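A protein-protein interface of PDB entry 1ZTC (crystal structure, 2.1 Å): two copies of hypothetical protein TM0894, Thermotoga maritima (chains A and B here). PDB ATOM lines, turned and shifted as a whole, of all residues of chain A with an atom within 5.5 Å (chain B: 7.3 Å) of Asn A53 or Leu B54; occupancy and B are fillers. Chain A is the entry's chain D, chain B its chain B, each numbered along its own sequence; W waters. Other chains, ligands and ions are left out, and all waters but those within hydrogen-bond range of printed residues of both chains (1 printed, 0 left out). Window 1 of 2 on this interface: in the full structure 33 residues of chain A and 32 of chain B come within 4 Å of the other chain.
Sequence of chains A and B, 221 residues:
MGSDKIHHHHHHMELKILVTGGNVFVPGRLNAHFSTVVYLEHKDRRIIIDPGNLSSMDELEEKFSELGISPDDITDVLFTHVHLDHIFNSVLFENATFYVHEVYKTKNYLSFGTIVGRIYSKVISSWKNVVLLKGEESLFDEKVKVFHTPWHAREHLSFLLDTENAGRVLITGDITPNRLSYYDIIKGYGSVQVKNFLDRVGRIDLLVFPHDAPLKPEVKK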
ATOM      1  N   ASN A  31       8.537 -16.510  31.428  1.00  0.00           N
ATOM      2  CA  ASN A  31       8.168 -15.170  31.750  1.00  0.00           C
ATOM      3  C   ASN A  31       7.209 -14.625  30.692  1.00  0.00           C
ATOM      4  O   ASN A  31       7.624 -14.177  29.624  1.00  0.00           O
ATOM      5  CB  ASN A  31       9.407 -14.305  31.853  1.00  0.00           C
ATOM      6  CG  ASN A  31       9.107 -12.922  32.384  1.00  0.00           C
ATOM      7  OD1 ASN A  31       8.008 -12.387  32.190  1.00  0.00           O
ATOM      8  ND2 ASN A  31      10.077 -12.348  33.081  1.00  0.00           N
ATOM      9  N   ALA A  32       5.924 -14.662  30.996  1.00  0.00           N
ATOM     10  CA  ALA A  32       4.927 -14.175  30.049  1.00  0.00           C
ATOM     11  C   ALA A  32       3.910 -13.251  30.723  1.00  0.00           C
ATOM     12  O   ALA A  32       2.725 -13.261  30.387  1.00  0.00           O
ATOM     13  CB  ALA A  32       4.236 -15.363  29.329  1.00  0.00           C
ATOM     14  N   HIS A  33       4.395 -12.426  31.645  1.00  0.00           N
ATOM     15  CA  HIS A  33       3.582 -11.355  32.197  1.00  0.00           C
ATOM     16  C   HIS A  33       3.041 -10.524  31.056  1.00  0.00           C
ATOM     17  O   HIS A  33       3.695 -10.328  30.013  1.00  0.00           O
ATOM     18  CB  HIS A  33       4.402 -10.451  33.112  1.00  0.00           C
ATOM     19  CG  HIS A  33       4.907 -11.114  34.345  1.00  0.00           C
ATOM     20  ND1 HIS A  33       4.092 -11.831  35.195  1.00  0.00           N
ATOM     21  CD2 HIS A  33       6.150 -11.154  34.890  1.00  0.00           C
ATOM     22  CE1 HIS A  33       4.806 -12.274  36.216  1.00  0.00           C
ATOM     23  NE2 HIS A  33       6.061 -11.888  36.050  1.00  0.00           N
ATOM     24  N   PHE A  34       1.845 -10.006  31.243  1.00  0.00           N
ATOM     25  CA  PHE A  34       1.198  -9.239  30.202  1.00  0.00           C
ATOM     26  C   PHE A  34       0.289  -8.193  30.850  1.00  0.00           C
ATOM     27  O   PHE A  34      -0.498  -8.508  31.739  1.00  0.00           O
ATOM     28  CB  PHE A  34       0.454 -10.178  29.223  1.00  0.00           C
ATOM     29  CG  PHE A  34      -0.702 -10.928  29.826  1.00  0.00           C
ATOM     30  CD1 PHE A  34      -0.483 -12.069  30.606  1.00  0.00           C
ATOM     31  CD2 PHE A  34      -2.022 -10.511  29.591  1.00  0.00           C
ATOM     32  CE1 PHE A  34      -1.564 -12.757  31.163  1.00  0.00           C
ATOM     33  CE2 PHE A  34      -3.098 -11.188  30.127  1.00  0.00           C
ATOM     34  CZ  PHE A  34      -2.871 -12.310  30.924  1.00  0.00           C
ATOM     35  N   SER A  35       0.446  -6.942  30.435  1.00  0.00           N
ATOM     36  CA  SER A  35      -0.320  -5.862  31.029  1.00  0.00           C
ATOM     37  C   SER A  35      -1.692  -5.732  30.374  1.00  0.00           C
ATOM     38  O   SER A  35      -1.946  -6.164  29.233  1.00  0.00           O
ATOM     39  CB  SER A  35       0.425  -4.523  30.955  1.00  0.00           C
ATOM     40  OG  SER A  35       0.308  -3.967  29.665  1.00  0.00           O
ATOM     41  N   PRO A  51       0.577  -0.816  25.640  1.00  0.00           N
ATOM     42  CA  PRO A  51       0.215  -1.704  24.537  1.00  0.00           C
ATOM     43  C   PRO A  51       0.357  -3.199  24.826  1.00  0.00           C
ATOM     44  O   PRO A  51      -0.213  -4.013  24.090  1.00  0.00           O
ATOM     45  CB  PRO A  51       1.118  -1.254  23.396  1.00  0.00           C
ATOM     46  CG  PRO A  51       2.194  -0.484  24.002  1.00  0.00           C
ATOM     47  CD  PRO A  51       1.703   0.065  25.294  1.00  0.00           C
ATOM     48  N   GLY A  52       1.106  -3.548  25.869  1.00  0.00           N
ATOM     49  CA  GLY A  52       1.145  -4.899  26.369  1.00  0.00           C
ATOM     50  C   GLY A  52       2.243  -5.774  25.805  1.00  0.00           C
ATOM     51  O   GLY A  52       3.200  -5.288  25.218  1.00  0.00           O
ATOM     52  N   ASN A  53       2.054  -7.076  25.965  1.00  0.00           N
ATOM     53  CA  ASN A  53       3.063  -8.068  25.663  1.00  0.00           C
ATOM     54  C   ASN A  53       2.632  -8.968  24.519  1.00  0.00           C
ATOM     55  O   ASN A  53       1.461  -9.025  24.170  1.00  0.00           O
ATOM     56  CB  ASN A  53       3.327  -8.923  26.896  1.00  0.00           C
ATOM     57  CG  ASN A  53       4.549  -9.798  26.785  1.00  0.00           C
ATOM     58  OD1 ASN A  53       5.643  -9.327  26.461  1.00  0.00           O
ATOM     59  ND2 ASN A  53       4.360 -11.113  27.067  1.00  0.00           N
ATOM     60  N   LEU A  54       3.617  -9.622  23.916  1.00  0.00           N
ATOM     61  CA  LEU A  54       3.438 -10.482  22.756  1.00  0.00           C
ATOM     62  C   LEU A  54       2.378 -11.546  22.991  1.00  0.00           C
ATOM     63  O   LEU A  54       1.641 -11.937  22.079  1.00  0.00           O
ATOM     64  CB  LEU A  54       4.792 -11.141  22.440  1.00  0.00           C
ATOM     65  CG  LEU A  54       4.927 -12.076  21.230  1.00  0.00           C
ATOM     66  CD1 LEU A  54       4.603 -11.327  19.980  1.00  0.00           C
ATOM     67  CD2 LEU A  54       6.339 -12.627  21.135  1.00  0.00           C
ATOM     68  N   SER A  55       2.274 -12.010  24.230  1.00  0.00           N
ATOM     69  CA  SER A  55       1.337 -13.087  24.542  1.00  0.00           C
ATOM     70  C   SER A  55      -0.162 -12.716  24.421  1.00  0.00           C
ATOM     71  O   SER A  55      -1.015 -13.611  24.358  1.00  0.00           O
ATOM     72  CB  SER A  55       1.658 -13.648  25.920  1.00  0.00           C
ATOM     73  OG  SER A  55       1.570 -12.650  26.896  1.00  0.00           O
ATOM     74  N   SER A  56      -0.449 -11.412  24.330  1.00  0.00           N
ATOM     75  CA  SER A  56      -1.795 -10.876  24.105  1.00  0.00           C
ATOM     76  C   SER A  56      -2.152 -10.684  22.625  1.00  0.00           C
ATOM     77  O   SER A  56      -3.188 -10.123  22.306  1.00  0.00           O
ATOM     78  CB  SER A  56      -1.929  -9.544  24.842  1.00  0.00           C
ATOM     79  OG  SER A  56      -2.021  -9.782  26.240  1.00  0.00           O
ATOM     80  N   MET A  57      -1.309 -11.175  21.725  1.00  0.00           N
ATOM     81  CA  MET A  57      -1.488 -10.937  20.299  1.00  0.00           C
ATOM     82  C   MET A  57      -2.837 -11.370  19.737  1.00  0.00           C
ATOM     83  O   MET A  57      -3.407 -10.640  18.939  1.00  0.00           O
ATOM     84  CB  MET A  57      -0.322 -11.531  19.479  1.00  0.00           C
ATOM     85  CG  MET A  57      -0.200 -13.041  19.543  1.00  0.00           C
ATOM     86  SD  MET A  57       1.437 -13.718  18.643  1.00  0.00           S
ATOM     87  CE  MET A  57       0.775 -15.448  18.548  1.00  0.00           C
ATOM     88  N   LEU A  60      -5.618  -9.035  21.085  1.00  0.00           N
ATOM     89  CA  LEU A  60      -5.554  -7.760  20.391  1.00  0.00           C
ATOM     90  C   LEU A  60      -6.043  -7.834  18.962  1.00  0.00           C
ATOM     91  O   LEU A  60      -6.755  -6.949  18.512  1.00  0.00           O
ATOM     92  CB  LEU A  60      -4.135  -7.191  20.408  1.00  0.00           C
ATOM     93  CG  LEU A  60      -3.715  -6.729  21.791  1.00  0.00           C
ATOM     94  CD1 LEU A  60      -2.227  -6.462  21.775  1.00  0.00           C
ATOM     95  CD2 LEU A  60      -4.518  -5.482  22.233  1.00  0.00           C
ATOM     96  N   LEU A  84       8.897  -4.611  29.904  1.00  0.00           N
ATOM     97  CA  LEU A  84       8.601  -5.264  28.631  1.00  0.00           C
ATOM     98  C   LEU A  84       7.157  -5.738  28.508  1.00  0.00           C
ATOM     99  O   LEU A  84       6.558  -5.736  27.433  1.00  0.00           O
ATOM    100  CB  LEU A  84       9.531  -6.456  28.486  1.00  0.00           C
ATOM    101  CG  LEU A  84       9.977  -6.807  27.082  1.00  0.00           C
ATOM    102  CD1 LEU A  84      10.620  -5.612  26.396  1.00  0.00           C
ATOM    103  CD2 LEU A  84      10.954  -7.966  27.206  1.00  0.00           C
ATOM    104  N   ASP A  85       6.602  -6.190  29.618  1.00  0.00           N
ATOM    105  CA  ASP A  85       5.240  -6.727  29.610  1.00  0.00           C
ATOM    106  C   ASP A  85       4.186  -5.647  29.404  1.00  0.00           C
ATOM    107  O   ASP A  85       3.023  -5.965  29.085  1.00  0.00           O
ATOM    108  CB  ASP A  85       4.973  -7.532  30.867  1.00  0.00           C
ATOM    109  CG  ASP A  85       5.186  -6.734  32.143  1.00  0.00           C
ATOM    110  OD1 ASP A  85       6.246  -6.054  32.283  1.00  0.00           O
ATOM    111  OD2 ASP A  85       4.276  -6.783  33.001  1.00  0.00           O
ATOM    112  N   HIS A  86       4.605  -4.382  29.521  1.00  0.00           N
ATOM    113  CA  HIS A  86       3.760  -3.220  29.232  1.00  0.00           C
ATOM    114  C   HIS A  86       4.040  -2.574  27.884  1.00  0.00           C
ATOM    115  O   HIS A  86       3.151  -1.961  27.307  1.00  0.00           O
ATOM    116  CB  HIS A  86       3.964  -2.144  30.295  1.00  0.00           C
ATOM    117  CG  HIS A  86       3.485  -2.541  31.641  1.00  0.00           C
ATOM    118  ND1 HIS A  86       2.418  -1.927  32.259  1.00  0.00           N
ATOM    119  CD2 HIS A  86       3.905  -3.512  32.481  1.00  0.00           C
ATOM    120  CE1 HIS A  86       2.209  -2.503  33.428  1.00  0.00           C
ATOM    121  NE2 HIS A  86       3.083  -3.475  33.575  1.00  0.00           N
ATOM    122  N   PHE A  88       6.053  -4.019  25.030  1.00  0.00           N
ATOM    123  CA  PHE A  88       6.552  -4.782  23.881  1.00  0.00           C
ATOM    124  C   PHE A  88       5.762  -4.450  22.597  1.00  0.00           C
ATOM    125  O   PHE A  88       6.341  -4.202  21.544  1.00  0.00           O
ATOM    126  CB  PHE A  88       6.537  -6.299  24.115  1.00  0.00           C
ATOM    127  CG  PHE A  88       6.981  -7.050  22.918  1.00  0.00           C
ATOM    128  CD1 PHE A  88       8.319  -7.291  22.704  1.00  0.00           C
ATOM    129  CD2 PHE A  88       6.072  -7.402  21.927  1.00  0.00           C
ATOM    130  CE1 PHE A  88       8.739  -7.897  21.539  1.00  0.00           C
ATOM    131  CE2 PHE A  88       6.496  -7.995  20.751  1.00  0.00           C
ATOM    132  CZ  PHE A  88       7.812  -8.262  20.564  1.00  0.00           C
ATOM    133  N   ASN A  89       4.443  -4.440  22.697  1.00  0.00           N
ATOM    134  CA  ASN A  89       3.604  -4.284  21.513  1.00  0.00           C
ATOM    135  C   ASN A  89       3.705  -2.894  20.877  1.00  0.00           C
ATOM    136  O   ASN A  89       3.154  -2.668  19.814  1.00  0.00           O
ATOM    137  CB  ASN A  89       2.134  -4.637  21.796  1.00  0.00           C
ATOM    138  CG  ASN A  89       1.935  -6.106  22.154  1.00  0.00           C
ATOM    139  OD1 ASN A  89       2.718  -6.959  21.746  1.00  0.00           O
ATOM    140  ND2 ASN A  89       0.862  -6.405  22.911  1.00  0.00           N
ATOM    141  N   ILE A 119      16.579  -6.962  23.906  1.00  0.00           N
ATOM    142  CA  ILE A 119      15.174  -6.831  23.565  1.00  0.00           C
ATOM    143  C   ILE A 119      14.631  -5.456  23.962  1.00  0.00           C
ATOM    144  O   ILE A 119      13.953  -4.803  23.186  1.00  0.00           O
ATOM    145  CB  ILE A 119      14.301  -7.918  24.250  1.00  0.00           C
ATOM    146  CG1 ILE A 119      14.789  -9.336  23.899  1.00  0.00           C
ATOM    147  CG2 ILE A 119      12.850  -7.738  23.828  1.00  0.00           C
ATOM    148  CD1 ILE A 119      14.749  -9.650  22.418  1.00  0.00           C
ATOM    149  N   LEU B  30      -4.244 -15.618  25.795  1.00  0.00           N
ATOM    150  CA  LEU B  30      -2.866 -15.842  26.146  1.00  0.00           C
ATOM    151  C   LEU B  30      -2.260 -16.829  25.215  1.00  0.00           C
ATOM    152  O   LEU B  30      -2.742 -17.963  25.053  1.00  0.00           O
ATOM    153  CB  LEU B  30      -2.734 -16.331  27.599  1.00  0.00           C
ATOM    154  CG  LEU B  30      -1.308 -16.569  28.136  1.00  0.00           C
ATOM    155  CD1 LEU B  30      -0.543 -15.267  28.266  1.00  0.00           C
ATOM    156  CD2 LEU B  30      -1.389 -17.242  29.496  1.00  0.00           C
ATOM    157  N   ASN B  31      -1.202 -16.386  24.555  1.00  0.00           N
ATOM    158  CA  ASN B  31      -0.447 -17.266  23.708  1.00  0.00           C
ATOM    159  C   ASN B  31       1.031 -17.131  24.041  1.00  0.00           C
ATOM    160  O   ASN B  31       1.691 -16.173  23.641  1.00  0.00           O
ATOM    161  CB  ASN B  31      -0.718 -16.962  22.258  1.00  0.00           C
ATOM    162  CG  ASN B  31      -0.075 -17.973  21.343  1.00  0.00           C
ATOM    163  OD1 ASN B  31       0.938 -18.605  21.696  1.00  0.00           O
ATOM    164  ND2 ASN B  31      -0.671 -18.157  20.170  1.00  0.00           N
ATOM    165  N   ALA B  32       1.549 -18.074  24.815  1.00  0.00           N
ATOM    166  CA  ALA B  32       2.953 -18.028  25.167  1.00  0.00           C
ATOM    167  C   ALA B  32       3.618 -19.382  24.967  1.00  0.00           C
ATOM    168  O   ALA B  32       4.516 -19.744  25.734  1.00  0.00           O
ATOM    169  CB  ALA B  32       3.120 -17.533  26.614  1.00  0.00           C
ATOM    170  N   HIS B  33       3.223 -20.097  23.913  1.00  0.00           N
ATOM    171  CA  HIS B  33       3.944 -21.296  23.498  1.00  0.00           C
ATOM    172  C   HIS B  33       5.420 -20.970  23.354  1.00  0.00           C
ATOM    173  O   HIS B  33       5.780 -19.867  23.000  1.00  0.00           O
ATOM    174  CB  HIS B  33       3.444 -21.825  22.181  1.00  0.00           C
ATOM    175  CG  HIS B  33       2.037 -22.312  22.219  1.00  0.00           C
ATOM    176  ND1 HIS B  33       1.577 -23.170  23.194  1.00  0.00           N
ATOM    177  CD2 HIS B  33       0.981 -22.050  21.410  1.00  0.00           C
ATOM    178  CE1 HIS B  33       0.300 -23.431  22.969  1.00  0.00           C
ATOM    179  NE2 HIS B  33      -0.088 -22.762  21.896  1.00  0.00           N
ATOM    180  N   PHE B  34       6.267 -21.933  23.671  1.00  0.00           N
ATOM    181  CA  PHE B  34       7.706 -21.726  23.613  1.00  0.00           C
ATOM    182  C   PHE B  34       8.398 -23.043  23.260  1.00  0.00           C
ATOM    183  O   PHE B  34       8.076 -24.091  23.798  1.00  0.00           O
ATOM    184  CB  PHE B  34       8.225 -21.092  24.929  1.00  0.00           C
ATOM    185  CG  PHE B  34       8.096 -21.967  26.138  1.00  0.00           C
ATOM    186  CD1 PHE B  34       6.896 -22.065  26.818  1.00  0.00           C
ATOM    187  CD2 PHE B  34       9.203 -22.652  26.637  1.00  0.00           C
ATOM    188  CE1 PHE B  34       6.792 -22.862  27.933  1.00  0.00           C
ATOM    189  CE2 PHE B  34       9.113 -23.447  27.751  1.00  0.00           C
ATOM    190  CZ  PHE B  34       7.904 -23.563  28.405  1.00  0.00           C
ATOM    191  N   PRO B  51      15.524 -21.056  18.067  1.00  0.00           N
ATOM    192  CA  PRO B  51      15.962 -20.156  19.132  1.00  0.00           C
ATOM    193  C   PRO B  51      14.865 -19.828  20.141  1.00  0.00           C
ATOM    194  O   PRO B  51      15.155 -19.299  21.227  1.00  0.00           O
ATOM    195  CB  PRO B  51      16.434 -18.899  18.363  1.00  0.00           C
ATOM    196  CG  PRO B  51      15.706 -18.946  17.072  1.00  0.00           C
ATOM    197  CD  PRO B  51      15.550 -20.392  16.751  1.00  0.00           C
ATOM    198  N   GLY B  52      13.617 -20.151  19.811  1.00  0.00           N
ATOM    199  CA  GLY B  52      12.550 -20.095  20.823  1.00  0.00           C
ATOM    200  C   GLY B  52      11.806 -18.779  20.910  1.00  0.00           C
ATOM    201  O   GLY B  52      11.896 -17.913  20.016  1.00  0.00           O
ATOM    202  N   ASN B  53      11.059 -18.635  22.009  1.00  0.00           N
ATOM    203  CA  ASN B  53      10.139 -17.523  22.183  1.00  0.00           C
ATOM    204  C   ASN B  53      10.584 -16.593  23.296  1.00  0.00           C
ATOM    205  O   ASN B  53      11.348 -16.952  24.192  1.00  0.00           O
ATOM    206  CB  ASN B  53       8.732 -18.041  22.431  1.00  0.00           C
ATOM    207  CG  ASN B  53       7.656 -17.010  22.134  1.00  0.00           C
ATOM    208  OD1 ASN B  53       7.838 -16.101  21.299  1.00  0.00           O
ATOM    209  ND2 ASN B  53       6.573 -17.081  22.894  1.00  0.00           N
ATOM    210  N   LEU B  54      10.074 -15.377  23.219  1.00  0.00           N
ATOM    211  CA  LEU B  54      10.378 -14.331  24.139  1.00  0.00           C
ATOM    212  C   LEU B  54      10.237 -14.765  25.610  1.00  0.00           C
ATOM    213  O   LEU B  54      11.044 -14.381  26.457  1.00  0.00           O
ATOM    214  CB  LEU B  54       9.469 -13.136  23.791  1.00  0.00           C
ATOM    215  CG  LEU B  54       9.590 -11.872  24.673  1.00  0.00           C
ATOM    216  CD1 LEU B  54      10.958 -11.222  24.553  1.00  0.00           C
ATOM    217  CD2 LEU B  54       8.475 -10.871  24.335  1.00  0.00           C
ATOM    218  N   SER B  55       9.256 -15.607  25.909  1.00  0.00           N
ATOM    219  CA  SER B  55       9.016 -16.036  27.278  1.00  0.00           C
ATOM    220  C   SER B  55      10.142 -16.860  27.933  1.00  0.00           C
ATOM    221  O   SER B  55      10.171 -17.011  29.169  1.00  0.00           O
ATOM    222  CB  SER B  55       7.689 -16.796  27.323  1.00  0.00           C
ATOM    223  OG  SER B  55       7.685 -17.889  26.455  1.00  0.00           O
ATOM    224  N   SER B  56      11.060 -17.373  27.110  1.00  0.00           N
ATOM    225  CA  SER B  56      12.242 -18.130  27.559  1.00  0.00           C
ATOM    226  C   SER B  56      13.452 -17.260  27.874  1.00  0.00           C
ATOM    227  O   SER B  56      14.548 -17.770  28.114  1.00  0.00           O
ATOM    228  CB  SER B  56      12.644 -19.152  26.479  1.00  0.00           C
ATOM    229  OG  SER B  56      11.692 -20.187  26.417  1.00  0.00           O
ATOM    230  N   MET B  57      13.266 -15.943  27.845  1.00  0.00           N
ATOM    231  CA  MET B  57      14.377 -15.001  27.948  1.00  0.00           C
ATOM    232  C   MET B  57      15.216 -15.142  29.219  1.00  0.00           C
ATOM    233  O   MET B  57      16.405 -15.003  29.143  1.00  0.00           O
ATOM    234  CB  MET B  57      13.902 -13.543  27.814  1.00  0.00           C
ATOM    235  CG  MET B  57      12.993 -13.048  28.933  1.00  0.00           C
ATOM    236  SD  MET B  57      12.229 -11.233  28.586  1.00  0.00           S
ATOM    237  CE  MET B  57      10.363 -11.718  28.947  1.00  0.00           C
ATOM    238  N   ASP B  58      14.595 -15.414  30.363  1.00  0.00           N
ATOM    239  CA  ASP B  58      15.337 -15.602  31.619  1.00  0.00           C
ATOM    240  C   ASP B  58      16.128 -16.914  31.615  1.00  0.00           C
ATOM    241  O   ASP B  58      17.244 -16.966  32.131  1.00  0.00           O
ATOM    242  CB  ASP B  58      14.423 -15.653  32.853  1.00  0.00           C
ATOM    243  CG  ASP B  58      13.651 -14.358  33.111  1.00  0.00           C
ATOM    244  OD1 ASP B  58      14.033 -13.304  32.562  1.00  0.00           O
ATOM    245  OD2 ASP B  58      12.661 -14.432  33.905  1.00  0.00           O
ATOM    246  N   LEU B  60      17.259 -18.463  28.947  1.00  0.00           N
ATOM    247  CA  LEU B  60      18.352 -18.277  27.987  1.00  0.00           C
ATOM    248  C   LEU B  60      19.465 -17.408  28.538  1.00  0.00           C
ATOM    249  O   LEU B  60      20.647 -17.699  28.337  1.00  0.00           O
ATOM    250  CB  LEU B  60      17.819 -17.700  26.691  1.00  0.00           C
ATOM    251  CG  LEU B  60      17.060 -18.741  25.864  1.00  0.00           C
ATOM    252  CD1 LEU B  60      16.284 -18.045  24.757  1.00  0.00           C
ATOM    253  CD2 LEU B  60      17.985 -19.819  25.300  1.00  0.00           C
ATOM    254  N   LEU B  84       6.141 -18.598  15.298  1.00  0.00           N
ATOM    255  CA  LEU B  84       6.715 -17.584  16.167  1.00  0.00           C
ATOM    256  C   LEU B  84       7.354 -18.144  17.435  1.00  0.00           C
ATOM    257  O   LEU B  84       8.405 -17.664  17.890  1.00  0.00           O
ATOM    258  CB  LEU B  84       5.623 -16.588  16.532  1.00  0.00           C
ATOM    259  CG  LEU B  84       6.091 -15.179  16.831  1.00  0.00           C
ATOM    260  CD1 LEU B  84       6.923 -14.608  15.709  1.00  0.00           C
ATOM    261  CD2 LEU B  84       4.853 -14.306  17.111  1.00  0.00           C
ATOM    262  N   ASP B  85       6.715 -19.169  18.009  1.00  0.00           N
ATOM    263  CA  ASP B  85       7.186 -19.767  19.256  1.00  0.00           C
ATOM    264  C   ASP B  85       8.521 -20.511  19.094  1.00  0.00           C
ATOM    265  O   ASP B  85       9.210 -20.780  20.084  1.00  0.00           O
ATOM    266  CB  ASP B  85       6.090 -20.639  19.878  1.00  0.00           C
ATOM    267  CG  ASP B  85       5.605 -21.734  18.942  1.00  0.00           C
ATOM    268  OD1 ASP B  85       5.288 -21.442  17.752  1.00  0.00           O
ATOM    269  OD2 ASP B  85       5.594 -22.891  19.394  1.00  0.00           O
ATOM    270  N   PHE B  88      11.081 -16.580  17.250  1.00  0.00           N
ATOM    271  CA  PHE B  88      11.092 -15.180  17.699  1.00  0.00           C
ATOM    272  C   PHE B  88      12.495 -14.720  18.095  1.00  0.00           C
ATOM    273  O   PHE B  88      12.941 -13.655  17.699  1.00  0.00           O
ATOM    274  CB  PHE B  88      10.157 -14.937  18.896  1.00  0.00           C
ATOM    275  CG  PHE B  88      10.210 -13.526  19.364  1.00  0.00           C
ATOM    276  CD1 PHE B  88       9.408 -12.560  18.771  1.00  0.00           C
ATOM    277  CD2 PHE B  88      11.161 -13.131  20.303  1.00  0.00           C
ATOM    278  CE1 PHE B  88       9.520 -11.233  19.134  1.00  0.00           C
ATOM    279  CE2 PHE B  88      11.278 -11.820  20.671  1.00  0.00           C
ATOM    280  CZ  PHE B  88      10.456 -10.864  20.084  1.00  0.00           C
ATOM    281  N   ASN B  89      13.196 -15.541  18.871  1.00  0.00           N
ATOM    282  CA  ASN B  89      14.479 -15.154  19.449  1.00  0.00           C
ATOM    283  C   ASN B  89      15.577 -15.033  18.417  1.00  0.00           C
ATOM    284  O   ASN B  89      16.691 -14.608  18.735  1.00  0.00           O
ATOM    285  CB  ASN B  89      14.879 -16.146  20.550  1.00  0.00           C
ATOM    286  CG  ASN B  89      14.007 -16.013  21.809  1.00  0.00           C
ATOM    287  OD1 ASN B  89      13.446 -14.955  22.067  1.00  0.00           O
ATOM    288  ND2 ASN B  89      13.926 -17.076  22.597  1.00  0.00           N
ATOM    289  N   VAL B  91      15.774 -12.790  16.423  1.00  0.00           N
ATOM    290  CA  VAL B  91      16.127 -11.355  16.393  1.00  0.00           C
ATOM    291  C   VAL B  91      17.374 -10.995  17.246  1.00  0.00           C
ATOM    292  O   VAL B  91      17.968  -9.930  17.065  1.00  0.00           O
ATOM    293  CB  VAL B  91      14.917 -10.447  16.803  1.00  0.00           C
ATOM    294  CG1 VAL B  91      13.711 -10.701  15.887  1.00  0.00           C
ATOM    295  CG2 VAL B  91      14.545 -10.643  18.263  1.00  0.00           C
HETATM  296  O   HOH W   1      -3.428 -13.724  23.002  1.00  0.00           O
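Among the printed residues, pairs that only touch across the chains: Ser A55 with Leu B30, Met A57 with Asn B31, Ala A32 with Ala B32, Phe A88 with Phe B88, Asn A31 with Met B57, Leu A84 with Met B57, Leu A54 with Asn B53, Met A57 with Leu B84, Asn A53 with Leu B54, Leu A54 with Phe B88, Phe A88 with Leu B54 and Phe A34 with Leu B30.
Water W1 lies within hydrogen-bond range of O of Ser A55 (2.8 Å) and N of Leu B30 (3.5 Å).
Asn A31 touches Ser B55, and with the chains exchanged Ser A55 touches Asn B31. Ala B32 touches its own counterpart, Ala A32. Leu A54 touches Phe B88, and with the chains exchanged Phe A88 touches Leu B54. Phe B88 touches its own counterpart, Phe A88. Of the 15 pairs that touch across the chains among the printed residues, 12 have their exchanged pair printed and touching as well.
Printed residues of chain B within 4 Å of Asn A53: Leu B54 (3.9 Å). Printed residues of chain A within 4 Å of Leu B54: Asn A53 (3.9 Å) and Phe A88 (3.9 Å). Of the printed residues of chain B, Met A57 touches Asn B31 and Leu B84. Of the printed residues of chain B, Leu A84 touches Met B57 (3.8 Å). Printed residues of chain A within 4 Å of Asp B58: Asn A31. The nearest printed residue of chain B that does not touch Asn A53 is Met B57 (5.8 Å). The nearest printed residue of chain A that does not touch Leu B54 is Ile A119 (4.03 Å). The nearest printed residue of chain A that does not touch Asn B53 is Ser A55 (6.7 Å).
Hydrophobic or aromatic side chains of chain B that line the printed part of chain A: Leu B30, Ala B32, Leu B54, Met B57, Leu B84 and Phe B88. Among the printed residues, 15 pairs touch across the chains.
O of Gly A52 sits at hydrogen-bond distance from N of Phe A88, 3.1 Å away. O of His A33 sits at hydrogen-bond distance from ND2 of Asn A53 (3.1 Å). The side-chain amide nitrogen (ND2) of Asn B53 lies within hydrogen-bond range of the backbone carbonyl oxygen (O) of His B33 (2.9 Å). The backbone carbonyl oxygen (O) of Gly B52 is in hydrogen-bond range of the backbone NH (N) of Phe B88, at 3.2 Å. The side-chain amide nitrogen (ND2) of Asn A53 lies within hydrogen-bond range of the side-chain hydroxyl (OG) of Ser A55, 3.2 Å away. The backbone carbonyl oxygen (O) of Asn A53 is in hydrogen-bond range of the side-chain amide nitrogen (ND2) of Asn A89 (3.0 Å).
The backbone NH of Asn A31 lies within hydrogen-bond range of the backbone carbonyl oxygen of Ser B55. N of Asn B31 is in hydrogen-bond range of O of Ser A55 (2.8 Å). The side-chain carboxylate of Asp B58 is in hydrogen-bond range of the side-chain amide nitrogen of Asn A31, at 3.4 Å.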
